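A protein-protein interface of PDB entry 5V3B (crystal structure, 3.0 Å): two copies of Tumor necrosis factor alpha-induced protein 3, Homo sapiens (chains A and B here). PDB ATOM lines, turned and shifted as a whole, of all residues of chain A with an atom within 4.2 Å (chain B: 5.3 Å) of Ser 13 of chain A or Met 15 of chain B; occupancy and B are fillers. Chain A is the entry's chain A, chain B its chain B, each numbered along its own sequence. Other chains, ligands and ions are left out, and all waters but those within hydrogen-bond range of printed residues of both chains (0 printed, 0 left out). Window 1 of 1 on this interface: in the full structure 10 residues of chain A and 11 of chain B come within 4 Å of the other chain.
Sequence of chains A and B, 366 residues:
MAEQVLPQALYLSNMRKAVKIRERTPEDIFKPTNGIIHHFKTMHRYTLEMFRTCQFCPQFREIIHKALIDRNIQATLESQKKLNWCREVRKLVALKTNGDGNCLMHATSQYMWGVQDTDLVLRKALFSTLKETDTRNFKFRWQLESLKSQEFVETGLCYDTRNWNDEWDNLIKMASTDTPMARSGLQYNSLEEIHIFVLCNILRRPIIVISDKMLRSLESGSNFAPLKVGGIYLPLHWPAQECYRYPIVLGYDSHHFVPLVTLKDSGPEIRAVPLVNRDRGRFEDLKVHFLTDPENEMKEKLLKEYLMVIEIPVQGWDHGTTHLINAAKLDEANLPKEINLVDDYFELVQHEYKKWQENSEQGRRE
The side-chain sulfur of Met 15 of chain A sits close to the backbone carbonyl oxygen of Leu 12 of chain B.
O of Ser 13 of chain B lies within hydrogen-bond range of N of Met 15 of chain A (3.5 Å).
The side-chain amide oxygen (OD1) of Asn 14 of chain B lies close to the side-chain amide nitrogen (ND2) of Asn 14 of chain A.
O of Ser 13 of chain A lies within hydrogen-bond range of N of Arg 16 of chain B (3.2 Å).
O of Ser 13 of chain A is in hydrogen-bond range of N of Met 15 of chain B (3.4 Å).
The backbone carbonyl oxygen of Leu 12 of chain A sits close to the side-chain sulfur of Met 15 of chain B (3.4 Å).
The side-chain amide nitrogen (ND2) of Asn 14 of chain A sits at hydrogen-bond distance from the side-chain carboxylate (OD2) of Asp 344 of chain A (2.7 Å).
The side-chain amide oxygen (OD1) of Asn 14 of chain B is in hydrogen-bond range of the backbone NH (N) of Lys 17 of chain B (3.1 Å).
OG of Ser 13 of chain A sits close to O of Leu 10 of chain A, at 3.4 Å.
The backbone NH (N) of Arg 16 of chain B lies close to the side-chain amide oxygen (OD1) of Asn 14 of chain B, 3.4 Å away.
N of Tyr 345 of chain A sits at hydrogen-bond distance from OG of Ser 13 of chain A, 3.1 Å away.
Asp 344 of chain A touches Arg 16 of chain B.
CD1 of Leu 348 of chain A touches CB of Met 15 of chain B, at 3.5 Å.
Ala 9 of chain A touches none of the printed residues of chain B.
Ser 13 of chain A touches two residues of chain B.
Printed residues of chain B within 4 Å of Asp 344 of chain A: Arg 16.
Of the printed residues of chain A, Asn 14 of chain B touches Asn 14 (3.2 Å).
Of the printed residues of chain A, Met 15 of chain B touches Leu 12 (3.4 Å), Ser 13 (3.4 Å) and Leu 348 (3.5 Å).
The nearest residue of chain B that does not touch Ser 13 of chain A is Asn 14 of chain B (4.2 Å).
Hydrophobic or aromatic side chains of chain A within 4 Å of the printed part of chain B: Met 15 and Leu 348.
Printed residues of chain B that touch a printed residue of chain A: Leu 12, Ser 13, Asn 14, Met 15 and Arg 16.
Among the printed residues, 8 pairs touch across the chains.
Among the printed residues, no Asp or Glu carboxylate lies within 4 Å of a Lys or Arg side-chain nitrogen of the other chain.
Leu 12 of chain A touches Met 15 of chain B, and with the chains exchanged Met 15 of chain A touches Leu 12 of chain B.
Ser 13 of chain A touches Met 15 of chain B, and with the chains exchanged Met 15 of chain A touches Ser 13 of chain B.
Asn 14 of chain B touches its own counterpart, Asn 14 of chain A.
5 positions are printed for both chains.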
ATOM      1  N   ALA A   9       1.183 -13.610  27.614  1.00  0.00           N
ATOM      2  CA  ALA A   9       0.157 -12.961  26.792  1.00  0.00           C
ATOM      3  C   ALA A   9      -0.050 -13.658  25.458  1.00  0.00           C
ATOM      4  O   ALA A   9       0.902 -14.238  24.907  1.00  0.00           O
ATOM      5  CB  ALA A   9       0.565 -11.527  26.561  1.00  0.00           C
ATOM      6  N   LEU A  10      -1.272 -13.579  24.920  1.00  0.00           N
ATOM      7  CA  LEU A  10      -1.593 -14.229  23.637  1.00  0.00           C
ATOM      8  C   LEU A  10      -0.585 -13.934  22.546  1.00  0.00           C
ATOM      9  O   LEU A  10      -0.188 -14.861  21.821  1.00  0.00           O
ATOM     10  CB  LEU A  10      -2.977 -13.789  23.135  1.00  0.00           C
ATOM     11  CG  LEU A  10      -4.135 -14.461  23.863  1.00  0.00           C
ATOM     12  CD1 LEU A  10      -5.448 -13.845  23.386  1.00  0.00           C
ATOM     13  CD2 LEU A  10      -4.147 -15.980  23.639  1.00  0.00           C
ATOM     14  N   TYR A  11      -0.153 -12.671  22.450  1.00  0.00           N
ATOM     15  CA  TYR A  11       0.671 -12.245  21.331  1.00  0.00           C
ATOM     16  C   TYR A  11       1.992 -13.021  21.280  1.00  0.00           C
ATOM     17  O   TYR A  11       2.444 -13.389  20.208  1.00  0.00           O
ATOM     18  CB  TYR A  11       0.898 -10.718  21.351  1.00  0.00           C
ATOM     19  CG  TYR A  11       2.176 -10.197  22.003  1.00  0.00           C
ATOM     20  CD1 TYR A  11       2.240 -10.018  23.370  1.00  0.00           C
ATOM     21  CD2 TYR A  11       3.291  -9.849  21.239  1.00  0.00           C
ATOM     22  CE1 TYR A  11       3.396  -9.503  23.987  1.00  0.00           C
ATOM     23  CE2 TYR A  11       4.433  -9.324  21.828  1.00  0.00           C
ATOM     24  CZ  TYR A  11       4.489  -9.150  23.210  1.00  0.00           C
ATOM     25  OH  TYR A  11       5.610  -8.653  23.853  1.00  0.00           O
ATOM     26  N   LEU A  12       2.572 -13.332  22.451  1.00  0.00           N
ATOM     27  CA  LEU A  12       3.852 -14.000  22.488  1.00  0.00           C
ATOM     28  C   LEU A  12       3.829 -15.430  21.938  1.00  0.00           C
ATOM     29  O   LEU A  12       4.880 -15.994  21.626  1.00  0.00           O
ATOM     30  CB  LEU A  12       4.366 -14.010  23.912  1.00  0.00           C
ATOM     31  CG  LEU A  12       4.630 -12.711  24.618  1.00  0.00           C
ATOM     32  CD1 LEU A  12       4.694 -12.880  26.124  1.00  0.00           C
ATOM     33  CD2 LEU A  12       5.897 -12.084  24.059  1.00  0.00           C
ATOM     34  N   SER A  13       2.640 -16.026  21.828  1.00  0.00           N
ATOM     35  CA  SER A  13       2.522 -17.340  21.191  1.00  0.00           C
ATOM     36  C   SER A  13       2.990 -17.347  19.738  1.00  0.00           C
ATOM     37  O   SER A  13       3.394 -18.390  19.275  1.00  0.00           O
ATOM     38  CB  SER A  13       1.085 -17.897  21.299  1.00  0.00           C
ATOM     39  OG  SER A  13       0.314 -17.724  20.120  1.00  0.00           O
ATOM     40  N   ASN A  14       2.914 -16.227  19.028  1.00  0.00           N
ATOM     41  CA  ASN A  14       3.374 -16.170  17.628  1.00  0.00           C
ATOM     42  C   ASN A  14       3.692 -14.731  17.178  1.00  0.00           C
ATOM     43  O   ASN A  14       2.989 -14.124  16.361  1.00  0.00           O
ATOM     44  CB  ASN A  14       2.309 -16.827  16.701  1.00  0.00           C
ATOM     45  CG  ASN A  14       2.759 -16.924  15.238  1.00  0.00           C
ATOM     46  OD1 ASN A  14       3.687 -16.244  14.796  1.00  0.00           O
ATOM     47  ND2 ASN A  14       2.107 -17.778  14.501  1.00  0.00           N
ATOM     48  N   MET A  15       4.794 -14.206  17.687  1.00  0.00           N
ATOM     49  CA  MET A  15       5.138 -12.800  17.441  1.00  0.00           C
ATOM     50  C   MET A  15       5.097 -12.368  15.983  1.00  0.00           C
ATOM     51  O   MET A  15       4.813 -11.198  15.704  1.00  0.00           O
ATOM     52  CB  MET A  15       6.495 -12.454  18.053  1.00  0.00           C
ATOM     53  CG  MET A  15       6.472 -12.413  19.586  1.00  0.00           C
ATOM     54  SD  MET A  15       8.111 -12.025  20.238  1.00  0.00           S
ATOM     55  CE  MET A  15       8.104 -10.207  20.160  1.00  0.00           C
ATOM     56  N   LEU A 341      -4.437 -15.330  16.847  1.00  0.00           N
ATOM     57  CA  LEU A 341      -3.431 -15.641  17.859  1.00  0.00           C
ATOM     58  C   LEU A 341      -3.926 -16.690  18.847  1.00  0.00           C
ATOM     59  O   LEU A 341      -3.134 -17.512  19.279  1.00  0.00           O
ATOM     60  CB  LEU A 341      -3.017 -14.392  18.622  1.00  0.00           C
ATOM     61  CG  LEU A 341      -2.109 -13.437  17.902  1.00  0.00           C
ATOM     62  CD1 LEU A 341      -2.246 -12.043  18.585  1.00  0.00           C
ATOM     63  CD2 LEU A 341      -0.649 -13.979  17.904  1.00  0.00           C
ATOM     64  N   ASP A 344      -3.219 -20.318  18.000  1.00  0.00           N
ATOM     65  CA  ASP A 344      -1.809 -20.620  18.214  1.00  0.00           C
ATOM     66  C   ASP A 344      -1.467 -20.864  19.684  1.00  0.00           C
ATOM     67  O   ASP A 344      -0.867 -21.872  20.018  1.00  0.00           O
ATOM     68  CB  ASP A 344      -0.900 -19.503  17.665  1.00  0.00           C
ATOM     69  CG  ASP A 344      -0.831 -19.466  16.138  1.00  0.00           C
ATOM     70  OD1 ASP A 344      -1.405 -20.371  15.456  1.00  0.00           O
ATOM     71  OD2 ASP A 344      -0.211 -18.528  15.613  1.00  0.00           O
ATOM     72  N   TYR A 345      -1.850 -19.954  20.561  1.00  0.00           N
ATOM     73  CA  TYR A 345      -1.623 -20.150  21.994  1.00  0.00           C
ATOM     74  C   TYR A 345      -2.209 -21.477  22.473  1.00  0.00           C
ATOM     75  O   TYR A 345      -1.624 -22.145  23.315  1.00  0.00           O
ATOM     76  CB  TYR A 345      -2.249 -19.013  22.800  1.00  0.00           C
ATOM     77  CG  TYR A 345      -1.735 -18.863  24.205  1.00  0.00           C
ATOM     78  CD1 TYR A 345      -2.236 -19.663  25.229  1.00  0.00           C
ATOM     79  CD2 TYR A 345      -0.785 -17.888  24.521  1.00  0.00           C
ATOM     80  CE1 TYR A 345      -1.788 -19.497  26.529  1.00  0.00           C
ATOM     81  CE2 TYR A 345      -0.345 -17.714  25.823  1.00  0.00           C
ATOM     82  CZ  TYR A 345      -0.841 -18.518  26.825  1.00  0.00           C
ATOM     83  OH  TYR A 345      -0.361 -18.372  28.105  1.00  0.00           O
ATOM     84  N   LEU A 348      -0.166 -24.433  21.559  1.00  0.00           N
ATOM     85  CA  LEU A 348       0.981 -24.340  22.450  1.00  0.00           C
ATOM     86  C   LEU A 348       0.657 -24.874  23.834  1.00  0.00           C
ATOM     87  O   LEU A 348       1.429 -25.645  24.383  1.00  0.00           O
ATOM     88  CB  LEU A 348       1.437 -22.890  22.538  1.00  0.00           C
ATOM     89  CG  LEU A 348       2.861 -22.612  22.953  1.00  0.00           C
ATOM     90  CD1 LEU A 348       3.305 -21.285  22.317  1.00  0.00           C
ATOM     91  CD2 LEU A 348       2.997 -22.619  24.489  1.00  0.00           C
ATOM     92  N   TYR B  11      13.598 -19.101  18.112  1.00  0.00           N
ATOM     93  CA  TYR B  11      12.368 -19.847  18.370  1.00  0.00           C
ATOM     94  C   TYR B  11      11.236 -18.937  18.851  1.00  0.00           C
ATOM     95  O   TYR B  11      10.098 -19.102  18.447  1.00  0.00           O
ATOM     96  CB  TYR B  11      12.619 -21.046  19.307  1.00  0.00           C
ATOM     97  CG  TYR B  11      12.348 -20.829  20.783  1.00  0.00           C
ATOM     98  CD1 TYR B  11      13.292 -20.210  21.612  1.00  0.00           C
ATOM     99  CD2 TYR B  11      11.159 -21.278  21.365  1.00  0.00           C
ATOM    100  CE1 TYR B  11      13.056 -20.027  22.970  1.00  0.00           C
ATOM    101  CE2 TYR B  11      10.917 -21.110  22.733  1.00  0.00           C
ATOM    102  CZ  TYR B  11      11.861 -20.477  23.531  1.00  0.00           C
ATOM    103  OH  TYR B  11      11.614 -20.298  24.880  1.00  0.00           O
ATOM    104  N   LEU B  12      11.565 -17.937  19.644  1.00  0.00           N
ATOM    105  CA  LEU B  12      10.549 -17.024  20.188  1.00  0.00           C
ATOM    106  C   LEU B  12       9.841 -16.178  19.122  1.00  0.00           C
ATOM    107  O   LEU B  12       8.775 -15.629  19.383  1.00  0.00           O
ATOM    108  CB  LEU B  12      11.190 -16.095  21.222  1.00  0.00           C
ATOM    109  CG  LEU B  12      11.817 -16.786  22.450  1.00  0.00           C
ATOM    110  CD1 LEU B  12      12.730 -15.815  23.184  1.00  0.00           C
ATOM    111  CD2 LEU B  12      10.745 -17.314  23.395  1.00  0.00           C
ATOM    112  N   SER B  13      10.420 -16.068  17.933  1.00  0.00           N
ATOM    113  CA  SER B  13       9.746 -15.383  16.826  1.00  0.00           C
ATOM    114  C   SER B  13       8.420 -16.038  16.436  1.00  0.00           C
ATOM    115  O   SER B  13       7.566 -15.358  15.920  1.00  0.00           O
ATOM    116  CB  SER B  13      10.653 -15.248  15.581  1.00  0.00           C
ATOM    117  OG  SER B  13      10.412 -16.230  14.588  1.00  0.00           O
ATOM    118  N   ASN B  14       8.257 -17.342  16.652  1.00  0.00           N
ATOM    119  CA  ASN B  14       7.009 -18.030  16.296  1.00  0.00           C
ATOM    120  C   ASN B  14       6.822 -19.329  17.102  1.00  0.00           C
ATOM    121  O   ASN B  14       6.854 -20.441  16.568  1.00  0.00           O
ATOM    122  CB  ASN B  14       6.945 -18.290  14.775  1.00  0.00           C
ATOM    123  CG  ASN B  14       5.588 -18.863  14.319  1.00  0.00           C
ATOM    124  OD1 ASN B  14       4.801 -19.367  15.119  1.00  0.00           O
ATOM    125  ND2 ASN B  14       5.328 -18.805  13.015  1.00  0.00           N
ATOM    126  N   MET B  15       6.551 -19.175  18.394  1.00  0.00           N
ATOM    127  CA  MET B  15       6.474 -20.331  19.278  1.00  0.00           C
ATOM    128  C   MET B  15       5.563 -21.464  18.789  1.00  0.00           C
ATOM    129  O   MET B  15       5.818 -22.618  19.103  1.00  0.00           O
ATOM    130  CB  MET B  15       6.074 -19.907  20.688  1.00  0.00           C
ATOM    131  CG  MET B  15       7.176 -19.168  21.438  1.00  0.00           C
ATOM    132  SD  MET B  15       6.570 -18.585  23.051  1.00  0.00           S
ATOM    133  CE  MET B  15       6.709 -20.043  24.109  1.00  0.00           C
ATOM    134  N   ARG B  16       4.519 -21.153  18.027  1.00  0.00           N
ATOM    135  CA  ARG B  16       3.689 -22.199  17.456  1.00  0.00           C
ATOM    136  C   ARG B  16       4.585 -23.026  16.558  1.00  0.00           C
ATOM    137  O   ARG B  16       4.773 -24.208  16.803  1.00  0.00           O
ATOM    138  CB  ARG B  16       2.496 -21.629  16.670  1.00  0.00           C
ATOM    139  CG  ARG B  16       1.690 -22.639  15.857  1.00  0.00           C
ATOM    140  CD  ARG B  16       1.089 -23.688  16.770  1.00  0.00           C
ATOM    141  NE  ARG B  16       0.177 -24.634  16.107  1.00  0.00           N
ATOM    142  CZ  ARG B  16       0.459 -25.887  15.758  1.00  0.00           C
ATOM    143  NH1 ARG B  16       1.674 -26.434  15.930  1.00  0.00           N
ATOM    144  NH2 ARG B  16      -0.511 -26.609  15.216  1.00  0.00           N
ATOM    145  N   LYS B  17       5.169 -22.388  15.551  1.00  0.00           N
ATOM    146  CA  LYS B  17       6.067 -23.064  14.597  1.00  0.00           C
ATOM    147  C   LYS B  17       7.134 -23.909  15.307  1.00  0.00           C
ATOM    148  O   LYS B  17       7.378 -25.063  14.937  1.00  0.00           O
ATOM    149  CB  LYS B  17       6.742 -22.038  13.675  1.00  0.00           C
ATOM    150  CG  LYS B  17       7.428 -22.635  12.467  1.00  0.00           C
ATOM    151  CD  LYS B  17       7.777 -21.588  11.417  1.00  0.00           C
ATOM    152  CE  LYS B  17       6.566 -21.154  10.583  1.00  0.00           C
ATOM    153  NZ  LYS B  17       6.873 -20.138   9.532  1.00  0.00           N
ATOM    154  N   ALA B  18       7.739 -23.341  16.350  1.00  0.00           N
ATOM    155  CA  ALA B  18       8.696 -24.077  17.150  1.00  0.00           C
ATOM    156  C   ALA B  18       8.138 -25.411  17.633  1.00  0.00           C
ATOM    157  O   ALA B  18       8.814 -26.425  17.529  1.00  0.00           O
ATOM    158  CB  ALA B  18       9.150 -23.246  18.335  1.00  0.00           C
ATOM    159  N   VAL B  19       6.909 -25.419  18.142  1.00  0.00           N
ATOM    160  CA  VAL B  19       6.299 -26.666  18.599  1.00  0.00           C
ATOM    161  C   VAL B  19       6.079 -27.659  17.452  1.00  0.00           C
ATOM    162  O   VAL B  19       6.367 -28.834  17.636  1.00  0.00           O
ATOM    163  CB  VAL B  19       4.978 -26.435  19.380  1.00  0.00           C
ATOM    164  CG1 VAL B  19       4.252 -27.752  19.685  1.00  0.00           C
ATOM    165  CG2 VAL B  19       5.271 -25.680  20.668  1.00  0.00           C
ATOM    166  N   ARG B  22       9.326 -29.376  17.297  1.00  0.00           N
ATOM    167  CA  ARG B  22       9.455 -30.231  18.461  1.00  0.00           C
ATOM    168  C   ARG B  22       8.519 -31.456  18.455  1.00  0.00           C
ATOM    169  O   ARG B  22       8.853 -32.495  19.028  1.00  0.00           O
ATOM    170  CB  ARG B  22       9.207 -29.444  19.747  1.00  0.00           C
ATOM    171  CG  ARG B  22      10.268 -28.410  20.092  1.00  0.00           C
ATOM    172  CD  ARG B  22       9.988 -27.849  21.469  1.00  0.00           C
ATOM    173  NE  ARG B  22      11.037 -26.953  21.900  1.00  0.00           N
ATOM    174  CZ  ARG B  22      11.028 -25.624  21.781  1.00  0.00           C
ATOM    175  NH1 ARG B  22       9.985 -24.964  21.247  1.00  0.00           N
ATOM    176  NH2 ARG B  22      12.079 -24.917  22.220  1.00  0.00           N
